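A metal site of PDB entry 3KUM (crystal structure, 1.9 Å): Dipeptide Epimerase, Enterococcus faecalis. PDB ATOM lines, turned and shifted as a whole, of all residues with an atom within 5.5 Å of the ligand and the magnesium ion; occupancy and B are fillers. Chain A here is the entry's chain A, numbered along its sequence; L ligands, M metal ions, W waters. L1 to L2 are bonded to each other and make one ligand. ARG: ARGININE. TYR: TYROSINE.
An oxygen (OH) of TYR L2 is in hydrogen-bond range of the side-chain carboxylate (OE1) of Glu 295, at 2.7 Å. The backbone carbonyl oxygen (O) of Cys 292 lies within hydrogen-bond range of a nitrogen (N) of TYR L2 (2.8 Å). OD2 of Asp 318 is in salt-bridge range of N of ARG L1 (2.8 Å). An oxygen (O) of TYR L2 lies within salt-bridge range of the side-chain amino group of Lys 159, 2.8 Å away. OG1 of Thr 134 is in hydrogen-bond range of N of ARG L1, 3.0 Å away. An oxygen (O) of TYR L2 lies within salt-bridge range of the side-chain amino group (NZ) of Lys 161 (3.7 Å). ND2 of Asn 191 sits close to OXT of TYR L2, at 3.1 Å. A nitrogen (N) of ARG L1 lies within salt-bridge range of the side-chain carboxylate (OD1) of Asp 320 (3.2 Å). The side-chain amino group (NZ) of Lys 264 is in salt-bridge range of an oxygen (O) of TYR L2.
NZ of Lys 159 lies within salt-bridge range of OE1 of Glu 215, 2.9 Å away. ND2 of Asn 262 sits close to OE2 of Glu 215 (3.1 Å). The side-chain carboxylate of Asp 189 lies within hydrogen-bond range of the backbone NH of Asn 191 (3.1 Å). N of Asp 240 lies within hydrogen-bond range of OE1 of Gln 216 (2.7 Å). SG of Cys 292 lies within hydrogen-bond range of OD1 of Asp 320. OD1 of Asp 318 sits at hydrogen-bond distance from OG1 of Thr 134, at 3.2 Å. The backbone NH (N) of Thr 134 sits at hydrogen-bond distance from the side-chain carboxylate (OD2) of Asp 320 (2.8 Å). The side-chain amide nitrogen (ND2) of Asn 191 lies within hydrogen-bond range of the side-chain carboxylate (OE2) of Glu 241.
Phe 19 touches the ligand. Ile 21 touches the ligand. Ile 26 touches the ligand. CZ of Phe 53 touches CE1 of TYR L2 (3.6 Å). Ile 54 touches the ligand. CB of Ala 294 touches OH of TYR L2, 3.1 Å away. Hydrophobic or aromatic side chains that line the ligand: Phe 19, Ile 21, Ile 26, Phe 53, Ile 54 and Ala 294. Along chain A the residues within 4 Å of the ligand span positions 19 to 320.
Residues that only touch the magnesium ion: Lys 159 (3.7 Å).
The magnesium ion is bound by water W3 (2.1 Å), OE2 of Glu 215 (2.1 Å), OD2 of Asp 189 (2.3 Å), OD2 of Asp 240 (2.4 Å) and OXT of TYR L2 (2.4 Å).
Water W3 lies within hydrogen-bond range of OE1 of Glu 241, OD1 of Asp 189 and ND2 of Asn 191.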
ATOM      1  N   PHE A  19      18.532  22.586  -3.958  1.00  0.00           N
ATOM      2  CA  PHE A  19      19.012  21.814  -2.813  1.00  0.00           C
ATOM      3  C   PHE A  19      19.334  20.376  -3.222  1.00  0.00           C
ATOM      4  O   PHE A  19      18.542  19.717  -3.891  1.00  0.00           O
ATOM      5  CB  PHE A  19      17.951  21.838  -1.709  1.00  0.00           C
ATOM      6  CG  PHE A  19      18.372  21.139  -0.444  1.00  0.00           C
ATOM      7  CD1 PHE A  19      19.504  21.556   0.264  1.00  0.00           C
ATOM      8  CD2 PHE A  19      17.615  20.081   0.060  1.00  0.00           C
ATOM      9  CE1 PHE A  19      19.877  20.924   1.455  1.00  0.00           C
ATOM     10  CE2 PHE A  19      17.982  19.441   1.248  1.00  0.00           C
ATOM     11  CZ  PHE A  19      19.116  19.861   1.942  1.00  0.00           C
ATOM     12  N   ILE A  21      20.885  16.432  -1.945  1.00  0.00           N
ATOM     13  CA  ILE A  21      21.229  15.466  -0.915  1.00  0.00           C
ATOM     14  C   ILE A  21      21.522  14.144  -1.618  1.00  0.00           C
ATOM     15  O   ILE A  21      21.353  14.032  -2.834  1.00  0.00           O
ATOM     16  CB  ILE A  21      20.082  15.267   0.122  1.00  0.00           C
ATOM     17  CG1 ILE A  21      18.893  14.559  -0.540  1.00  0.00           C
ATOM     18  CG2 ILE A  21      19.646  16.609   0.683  1.00  0.00           C
ATOM     19  CD1 ILE A  21      17.812  14.141   0.465  1.00  0.00           C
ATOM     20  N   ILE A  26      16.152  19.094  -5.557  1.00  0.00           N
ATOM     21  CA  ILE A  26      14.861  19.776  -5.610  1.00  0.00           C
ATOM     22  C   ILE A  26      15.097  21.270  -5.845  1.00  0.00           C
ATOM     23  O   ILE A  26      16.059  21.827  -5.334  1.00  0.00           O
ATOM     24  CB  ILE A  26      14.084  19.599  -4.273  1.00  0.00           C
ATOM     25  CG1 ILE A  26      12.795  20.425  -4.302  1.00  0.00           C
ATOM     26  CG2 ILE A  26      14.969  20.036  -3.102  1.00  0.00           C
ATOM     27  CD1 ILE A  26      12.024  20.387  -2.994  1.00  0.00           C
ATOM     28  N   GLY A  51       7.405  14.247  -0.480  1.00  0.00           N
ATOM     29  CA  GLY A  51       8.786  14.081  -0.921  1.00  0.00           C
ATOM     30  C   GLY A  51       8.921  12.749  -1.635  1.00  0.00           C
ATOM     31  O   GLY A  51       9.166  11.723  -0.982  1.00  0.00           O
ATOM     32  N   PHE A  53      11.233  11.199  -3.209  1.00  0.00           N
ATOM     33  CA  PHE A  53      12.374  10.337  -2.890  1.00  0.00           C
ATOM     34  C   PHE A  53      12.605  10.059  -1.409  1.00  0.00           C
ATOM     35  O   PHE A  53      13.616   9.472  -1.043  1.00  0.00           O
ATOM     36  CB  PHE A  53      13.674  10.847  -3.554  1.00  0.00           C
ATOM     37  CG  PHE A  53      14.052  12.256  -3.227  1.00  0.00           C
ATOM     38  CD1 PHE A  53      14.192  13.185  -4.249  1.00  0.00           C
ATOM     39  CD2 PHE A  53      14.330  12.645  -1.925  1.00  0.00           C
ATOM     40  CE1 PHE A  53      14.610  14.494  -3.977  1.00  0.00           C
ATOM     41  CE2 PHE A  53      14.757  13.942  -1.640  1.00  0.00           C
ATOM     42  CZ  PHE A  53      14.897  14.872  -2.662  1.00  0.00           C
ATOM     43  N   ILE A  54      11.656  10.459  -0.563  1.00  0.00           N
ATOM     44  CA  ILE A  54      11.749  10.197   0.874  1.00  0.00           C
ATOM     45  C   ILE A  54      10.606   9.248   1.266  1.00  0.00           C
ATOM     46  O   ILE A  54      10.836   8.178   1.830  1.00  0.00           O
ATOM     47  CB  ILE A  54      11.575  11.487   1.725  1.00  0.00           C
ATOM     48  CG1 ILE A  54      12.621  12.530   1.347  1.00  0.00           C
ATOM     49  CG2 ILE A  54      11.691  11.124   3.207  1.00  0.00           C
ATOM     50  CD1 ILE A  54      14.029  12.205   1.822  1.00  0.00           C
ATOM     51  N   THR A 134      20.608  23.817   7.303  1.00  0.00           N
ATOM     52  CA  THR A 134      21.274  22.785   6.525  1.00  0.00           C
ATOM     53  C   THR A 134      22.106  23.344   5.375  1.00  0.00           C
ATOM     54  O   THR A 134      21.875  24.459   4.897  1.00  0.00           O
ATOM     55  CB  THR A 134      20.232  21.777   5.946  1.00  0.00           C
ATOM     56  OG1 THR A 134      19.401  21.292   7.012  1.00  0.00           O
ATOM     57  CG2 THR A 134      20.927  20.594   5.297  1.00  0.00           C
ATOM     58  N   LYS A 159      23.780  21.716   9.781  1.00  0.00           N
ATOM     59  CA  LYS A 159      23.502  20.348   9.365  1.00  0.00           C
ATOM     60  C   LYS A 159      24.217  20.192   8.025  1.00  0.00           C
ATOM     61  O   LYS A 159      23.997  20.969   7.103  1.00  0.00           O
ATOM     62  CB  LYS A 159      21.995  20.123   9.194  1.00  0.00           C
ATOM     63  CG  LYS A 159      21.627  18.704   8.777  1.00  0.00           C
ATOM     64  CD  LYS A 159      20.136  18.415   8.928  1.00  0.00           C
ATOM     65  CE  LYS A 159      19.825  16.979   8.547  1.00  0.00           C
ATOM     66  NZ  LYS A 159      18.402  16.603   8.784  1.00  0.00           N
ATOM     67  N   LYS A 161      25.127  17.810   4.712  1.00  0.00           N
ATOM     68  CA  LYS A 161      24.791  16.650   3.893  1.00  0.00           C
ATOM     69  C   LYS A 161      26.039  16.057   3.262  1.00  0.00           C
ATOM     70  O   LYS A 161      26.961  16.768   2.861  1.00  0.00           O
ATOM     71  CB  LYS A 161      23.804  17.048   2.790  1.00  0.00           C
ATOM     72  CG  LYS A 161      22.413  17.473   3.290  1.00  0.00           C
ATOM     73  CD  LYS A 161      21.603  16.261   3.750  1.00  0.00           C
ATOM     74  CE  LYS A 161      20.213  16.675   4.210  1.00  0.00           C
ATOM     75  NZ  LYS A 161      19.393  15.508   4.644  1.00  0.00           N
ATOM     76  N   ASP A 189      24.470  14.344   7.878  1.00  0.00           N
ATOM     77  CA  ASP A 189      23.352  13.564   7.360  1.00  0.00           C
ATOM     78  C   ASP A 189      23.808  12.906   6.053  1.00  0.00           C
ATOM     79  O   ASP A 189      24.047  13.601   5.070  1.00  0.00           O
ATOM     80  CB  ASP A 189      22.158  14.472   7.088  1.00  0.00           C
ATOM     81  CG  ASP A 189      20.875  13.707   6.869  1.00  0.00           C
ATOM     82  OD1 ASP A 189      20.939  12.515   6.491  1.00  0.00           O
ATOM     83  OD2 ASP A 189      19.788  14.293   7.061  1.00  0.00           O
ATOM     84  N   ASN A 191      21.986  10.557   4.395  1.00  0.00           N
ATOM     85  CA  ASN A 191      20.824  10.005   3.721  1.00  0.00           C
ATOM     86  C   ASN A 191      21.008   8.595   3.144  1.00  0.00           C
ATOM     87  O   ASN A 191      20.886   8.392   1.936  1.00  0.00           O
ATOM     88  CB  ASN A 191      20.337  10.946   2.626  1.00  0.00           C
ATOM     89  CG  ASN A 191      19.602  12.145   3.182  1.00  0.00           C
ATOM     90  OD1 ASN A 191      20.136  13.257   3.245  1.00  0.00           O
ATOM     91  ND2 ASN A 191      18.361  11.931   3.624  1.00  0.00           N
ATOM     92  N   GLU A 215      23.317  11.371  11.094  1.00  0.00           N
ATOM     93  CA  GLU A 215      21.960  10.993  10.734  1.00  0.00           C
ATOM     94  C   GLU A 215      21.857   9.971   9.602  1.00  0.00           C
ATOM     95  O   GLU A 215      22.482  10.120   8.549  1.00  0.00           O
ATOM     96  CB  GLU A 215      21.188  12.269  10.335  1.00  0.00           C
ATOM     97  CG  GLU A 215      19.684  12.118  10.170  1.00  0.00           C
ATOM     98  CD  GLU A 215      18.983  13.465  10.013  1.00  0.00           C
ATOM     99  OE1 GLU A 215      19.598  14.503  10.332  1.00  0.00           O
ATOM    100  OE2 GLU A 215      17.810  13.477   9.582  1.00  0.00           O
ATOM    101  N   GLN A 216      21.081   8.913   9.849  1.00  0.00           N
ATOM    102  CA  GLN A 216      20.833   7.838   8.885  1.00  0.00           C
ATOM    103  C   GLN A 216      22.004   7.500   7.963  1.00  0.00           C
ATOM    104  O   GLN A 216      21.975   7.789   6.762  1.00  0.00           O
ATOM    105  CB  GLN A 216      19.602   8.190   8.019  1.00  0.00           C
ATOM    106  CG  GLN A 216      18.959   6.997   7.326  1.00  0.00           C
ATOM    107  CD  GLN A 216      18.264   6.055   8.297  1.00  0.00           C
ATOM    108  OE1 GLN A 216      17.555   6.505   9.196  1.00  0.00           O
ATOM    109  NE2 GLN A 216      18.459   4.753   8.109  1.00  0.00           N
ATOM    110  N   ASP A 240      16.459   8.531  10.698  1.00  0.00           N
ATOM    111  CA  ASP A 240      15.506   9.423  10.059  1.00  0.00           C
ATOM    112  C   ASP A 240      14.560   8.593   9.188  1.00  0.00           C
ATOM    113  O   ASP A 240      13.449   8.257   9.630  1.00  0.00           O
ATOM    114  CB  ASP A 240      16.230  10.485   9.222  1.00  0.00           C
ATOM    115  CG  ASP A 240      15.258  11.457   8.549  1.00  0.00           C
ATOM    116  OD1 ASP A 240      14.081  11.542   8.977  1.00  0.00           O
ATOM    117  OD2 ASP A 240      15.678  12.160   7.603  1.00  0.00           O
ATOM    118  N   GLU A 241      15.000   8.244   7.990  1.00  0.00           N
ATOM    119  CA  GLU A 241      14.175   7.458   7.080  1.00  0.00           C
ATOM    120  C   GLU A 241      13.813   6.078   7.619  1.00  0.00           C
ATOM    121  O   GLU A 241      12.864   5.456   7.145  1.00  0.00           O
ATOM    122  CB  GLU A 241      14.872   7.327   5.713  1.00  0.00           C
ATOM    123  CG  GLU A 241      15.121   8.651   5.003  1.00  0.00           C
ATOM    124  CD  GLU A 241      16.565   9.136   5.134  1.00  0.00           C
ATOM    125  OE1 GLU A 241      17.054   9.265   6.274  1.00  0.00           O
ATOM    126  OE2 GLU A 241      17.207   9.378   4.079  1.00  0.00           O
ATOM    127  N   ASN A 262      14.830  11.295  14.450  1.00  0.00           N
ATOM    128  CA  ASN A 262      14.346  12.498  13.768  1.00  0.00           C
ATOM    129  C   ASN A 262      12.856  12.344  13.456  1.00  0.00           C
ATOM    130  O   ASN A 262      12.431  11.373  12.819  1.00  0.00           O
ATOM    131  CB  ASN A 262      15.115  12.711  12.455  1.00  0.00           C
ATOM    132  CG  ASN A 262      14.596  13.904  11.667  1.00  0.00           C
ATOM    133  OD1 ASN A 262      13.397  14.057  11.455  1.00  0.00           O
ATOM    134  ND2 ASN A 262      15.514  14.751  11.197  1.00  0.00           N
ATOM    135  N   LYS A 264       9.396  13.934  11.695  1.00  0.00           N
ATOM    136  CA  LYS A 264       8.914  14.846  10.661  1.00  0.00           C
ATOM    137  C   LYS A 264       7.408  14.645  10.556  1.00  0.00           C
ATOM    138  O   LYS A 264       6.939  13.516  10.419  1.00  0.00           O
ATOM    139  CB  LYS A 264       9.551  14.550   9.291  1.00  0.00           C
ATOM    140  CG  LYS A 264      10.995  15.000   9.122  1.00  0.00           C
ATOM    141  CD  LYS A 264      11.457  14.742   7.692  1.00  0.00           C
ATOM    142  CE  LYS A 264      12.930  15.054   7.485  1.00  0.00           C
ATOM    143  NZ  LYS A 264      13.792  14.135   8.262  1.00  0.00           N
ATOM    144  N   CYS A 292      12.239  18.516   8.783  1.00  0.00           N
ATOM    145  CA  CYS A 292      11.302  19.003   7.787  1.00  0.00           C
ATOM    146  C   CYS A 292      11.676  18.544   6.398  1.00  0.00           C
ATOM    147  O   CYS A 292      12.808  18.125   6.162  1.00  0.00           O
ATOM    148  CB  CYS A 292      11.237  20.541   7.803  1.00  0.00           C
ATOM    149  SG  CYS A 292      12.789  21.377   7.326  1.00  0.00           S
ATOM    150  N   MET A 293      10.717  18.622   5.483  1.00  0.00           N
ATOM    151  CA  MET A 293      10.925  18.235   4.088  1.00  0.00           C
ATOM    152  C   MET A 293      11.299  19.513   3.361  1.00  0.00           C
ATOM    153  O   MET A 293      10.938  20.602   3.796  1.00  0.00           O
ATOM    154  CB  MET A 293       9.628  17.677   3.483  1.00  0.00           C
ATOM    155  CG  MET A 293       9.035  16.495   4.216  1.00  0.00           C
ATOM    156  SD  MET A 293      10.050  15.052   4.066  1.00  0.00           S
ATOM    157  CE  MET A 293       9.138  14.105   2.844  1.00  0.00           C
ATOM    158  N   ALA A 294      12.015  19.381   2.251  1.00  0.00           N
ATOM    159  CA  ALA A 294      12.386  20.551   1.471  1.00  0.00           C
ATOM    160  C   ALA A 294      11.149  21.154   0.805  1.00  0.00           C
ATOM    161  O   ALA A 294      11.104  22.363   0.559  1.00  0.00           O
ATOM    162  CB  ALA A 294      13.411  20.158   0.403  1.00  0.00           C
ATOM    163  N   GLU A 295      10.138  20.317   0.553  1.00  0.00           N
ATOM    164  CA  GLU A 295       8.900  20.765  -0.087  1.00  0.00           C
ATOM    165  C   GLU A 295       7.831  21.394   0.804  1.00  0.00           C
ATOM    166  O   GLU A 295       6.770  21.783   0.309  1.00  0.00           O
ATOM    167  CB  GLU A 295       8.262  19.601  -0.860  1.00  0.00           C
ATOM    168  CG  GLU A 295       9.173  18.960  -1.882  1.00  0.00           C
ATOM    169  CD  GLU A 295       9.718  17.629  -1.416  1.00  0.00           C
ATOM    170  OE1 GLU A 295      10.079  17.513  -0.216  1.00  0.00           O
ATOM    171  OE2 GLU A 295       9.794  16.691  -2.245  1.00  0.00           O
ATOM    172  N   ASP A 318      15.523  21.107  13.286  1.00  0.00           N
ATOM    173  CA  ASP A 318      16.029  21.311  11.927  1.00  0.00           C
ATOM    174  C   ASP A 318      14.829  21.799  11.119  1.00  0.00           C
ATOM    175  O   ASP A 318      14.279  21.076  10.293  1.00  0.00           O
ATOM    176  CB  ASP A 318      16.573  19.995  11.362  1.00  0.00           C
ATOM    177  CG  ASP A 318      17.021  20.122   9.912  1.00  0.00           C
ATOM    178  OD1 ASP A 318      17.505  21.202   9.533  1.00  0.00           O
ATOM    179  OD2 ASP A 318      16.916  19.118   9.157  1.00  0.00           O
ATOM    180  N   ASP A 320      14.377  24.585   8.816  1.00  0.00           N
ATOM    181  CA  ASP A 320      14.940  25.609   7.946  1.00  0.00           C
ATOM    182  C   ASP A 320      14.319  25.683   6.551  1.00  0.00           C
ATOM    183  O   ASP A 320      14.886  26.311   5.651  1.00  0.00           O
ATOM    184  CB  ASP A 320      16.441  25.354   7.795  1.00  0.00           C
ATOM    185  CG  ASP A 320      16.728  23.990   7.206  1.00  0.00           C
ATOM    186  OD1 ASP A 320      15.826  23.119   7.225  1.00  0.00           O
ATOM    187  OD2 ASP A 320      17.860  23.773   6.733  1.00  0.00           O
ATOM    188  N   ALA A 321      13.165  25.055   6.371  1.00  0.00           N
ATOM    189  CA  ALA A 321      12.507  25.068   5.065  1.00  0.00           C
ATOM    190  C   ALA A 321      12.137  26.482   4.588  1.00  0.00           C
ATOM    191  O   ALA A 321      12.283  26.804   3.406  1.00  0.00           O
ATOM    192  CB  ALA A 321      11.260  24.183   5.104  1.00  0.00           C
ATOM    193  N   PHE A 323      13.625  29.277   5.086  1.00  0.00           N
ATOM    194  CA  PHE A 323      14.787  30.108   4.756  1.00  0.00           C
ATOM    195  C   PHE A 323      15.129  30.104   3.273  1.00  0.00           C
ATOM    196  O   PHE A 323      15.746  31.044   2.771  1.00  0.00           O
ATOM    197  CB  PHE A 323      16.030  29.642   5.526  1.00  0.00           C
ATOM    198  CG  PHE A 323      15.839  29.531   7.015  1.00  0.00           C
ATOM    199  CD1 PHE A 323      14.878  30.308   7.669  1.00  0.00           C
ATOM    200  CD2 PHE A 323      16.644  28.676   7.769  1.00  0.00           C
ATOM    201  CE1 PHE A 323      14.721  30.230   9.047  1.00  0.00           C
ATOM    202  CE2 PHE A 323      16.485  28.585   9.151  1.00  0.00           C
ATOM    203  CZ  PHE A 323      15.520  29.368   9.798  1.00  0.00           C
ATOM    204  N   GLY A 324      14.729  29.048   2.574  1.00  0.00           N
ATOM    205  CA  GLY A 324      15.015  28.955   1.154  1.00  0.00           C
ATOM    206  C   GLY A 324      13.886  29.362   0.226  1.00  0.00           C
ATOM    207  O   GLY A 324      14.068  29.341  -0.987  1.00  0.00           O
HETATM  208  N   ARG L   1      16.729  20.128   6.509  1.00  0.00           N
HETATM  209  CA  ARG L   1      15.755  19.476   5.577  1.00  0.00           C
HETATM  210  C   ARG L   1      16.177  18.041   5.300  1.00  0.00           C
HETATM  211  O   ARG L   1      17.367  17.722   5.295  1.00  0.00           O
HETATM  212  CB  ARG L   1      15.694  20.243   4.258  1.00  0.00           C
HETATM  213  CG  ARG L   1      15.622  21.734   4.401  1.00  0.00           C
HETATM  214  CD  ARG L   1      16.083  22.388   3.115  1.00  0.00           C
HETATM  215  NE  ARG L   1      16.465  23.778   3.319  1.00  0.00           N
HETATM  216  CZ  ARG L   1      17.183  24.489   2.455  1.00  0.00           C
HETATM  217  NH1 ARG L   1      17.594  23.924   1.320  1.00  0.00           N
HETATM  218  NH2 ARG L   1      17.484  25.747   2.712  1.00  0.00           N
HETATM  219  N   TYR L   2      15.194  17.182   5.054  1.00  0.00           N
HETATM  220  CA  TYR L   2      15.456  15.781   4.763  1.00  0.00           C
HETATM  221  C   TYR L   2      16.368  15.104   5.785  1.00  0.00           C
HETATM  222  O   TYR L   2      16.490  15.630   6.908  1.00  0.00           O
HETATM  223  CB  TYR L   2      16.078  15.654   3.361  1.00  0.00           C
HETATM  224  CG  TYR L   2      15.166  16.093   2.245  1.00  0.00           C
HETATM  225  CD1 TYR L   2      15.677  16.777   1.148  1.00  0.00           C
HETATM  226  CD2 TYR L   2      13.790  15.829   2.283  1.00  0.00           C
HETATM  227  CE1 TYR L   2      14.861  17.191   0.111  1.00  0.00           C
HETATM  228  CE2 TYR L   2      12.957  16.244   1.243  1.00  0.00           C
HETATM  229  CZ  TYR L   2      13.500  16.923   0.166  1.00  0.00           C
HETATM  230  OH  TYR L   2      12.702  17.373  -0.865  1.00  0.00           O
HETATM  231  OXT TYR L   2      16.907  14.030   5.441  1.00  0.00           O
HETATM  232 MG    MG M   1      17.874  13.161   7.509  1.00  0.00          MG
HETATM  233  O   HOH W   1      18.422  28.111   3.021  1.00  0.00           O
HETATM  234  O   HOH W   2      15.385  24.821   0.389  1.00  0.00           O
HETATM  235  O   HOH W   3      18.559  11.299   6.932  1.00  0.00           O
HETATM  236  O   HOH W   4      13.954  12.426   5.371  1.00  0.00           O
HETATM  237  O   HOH W   5      15.026  17.157   8.892  1.00  0.00           O
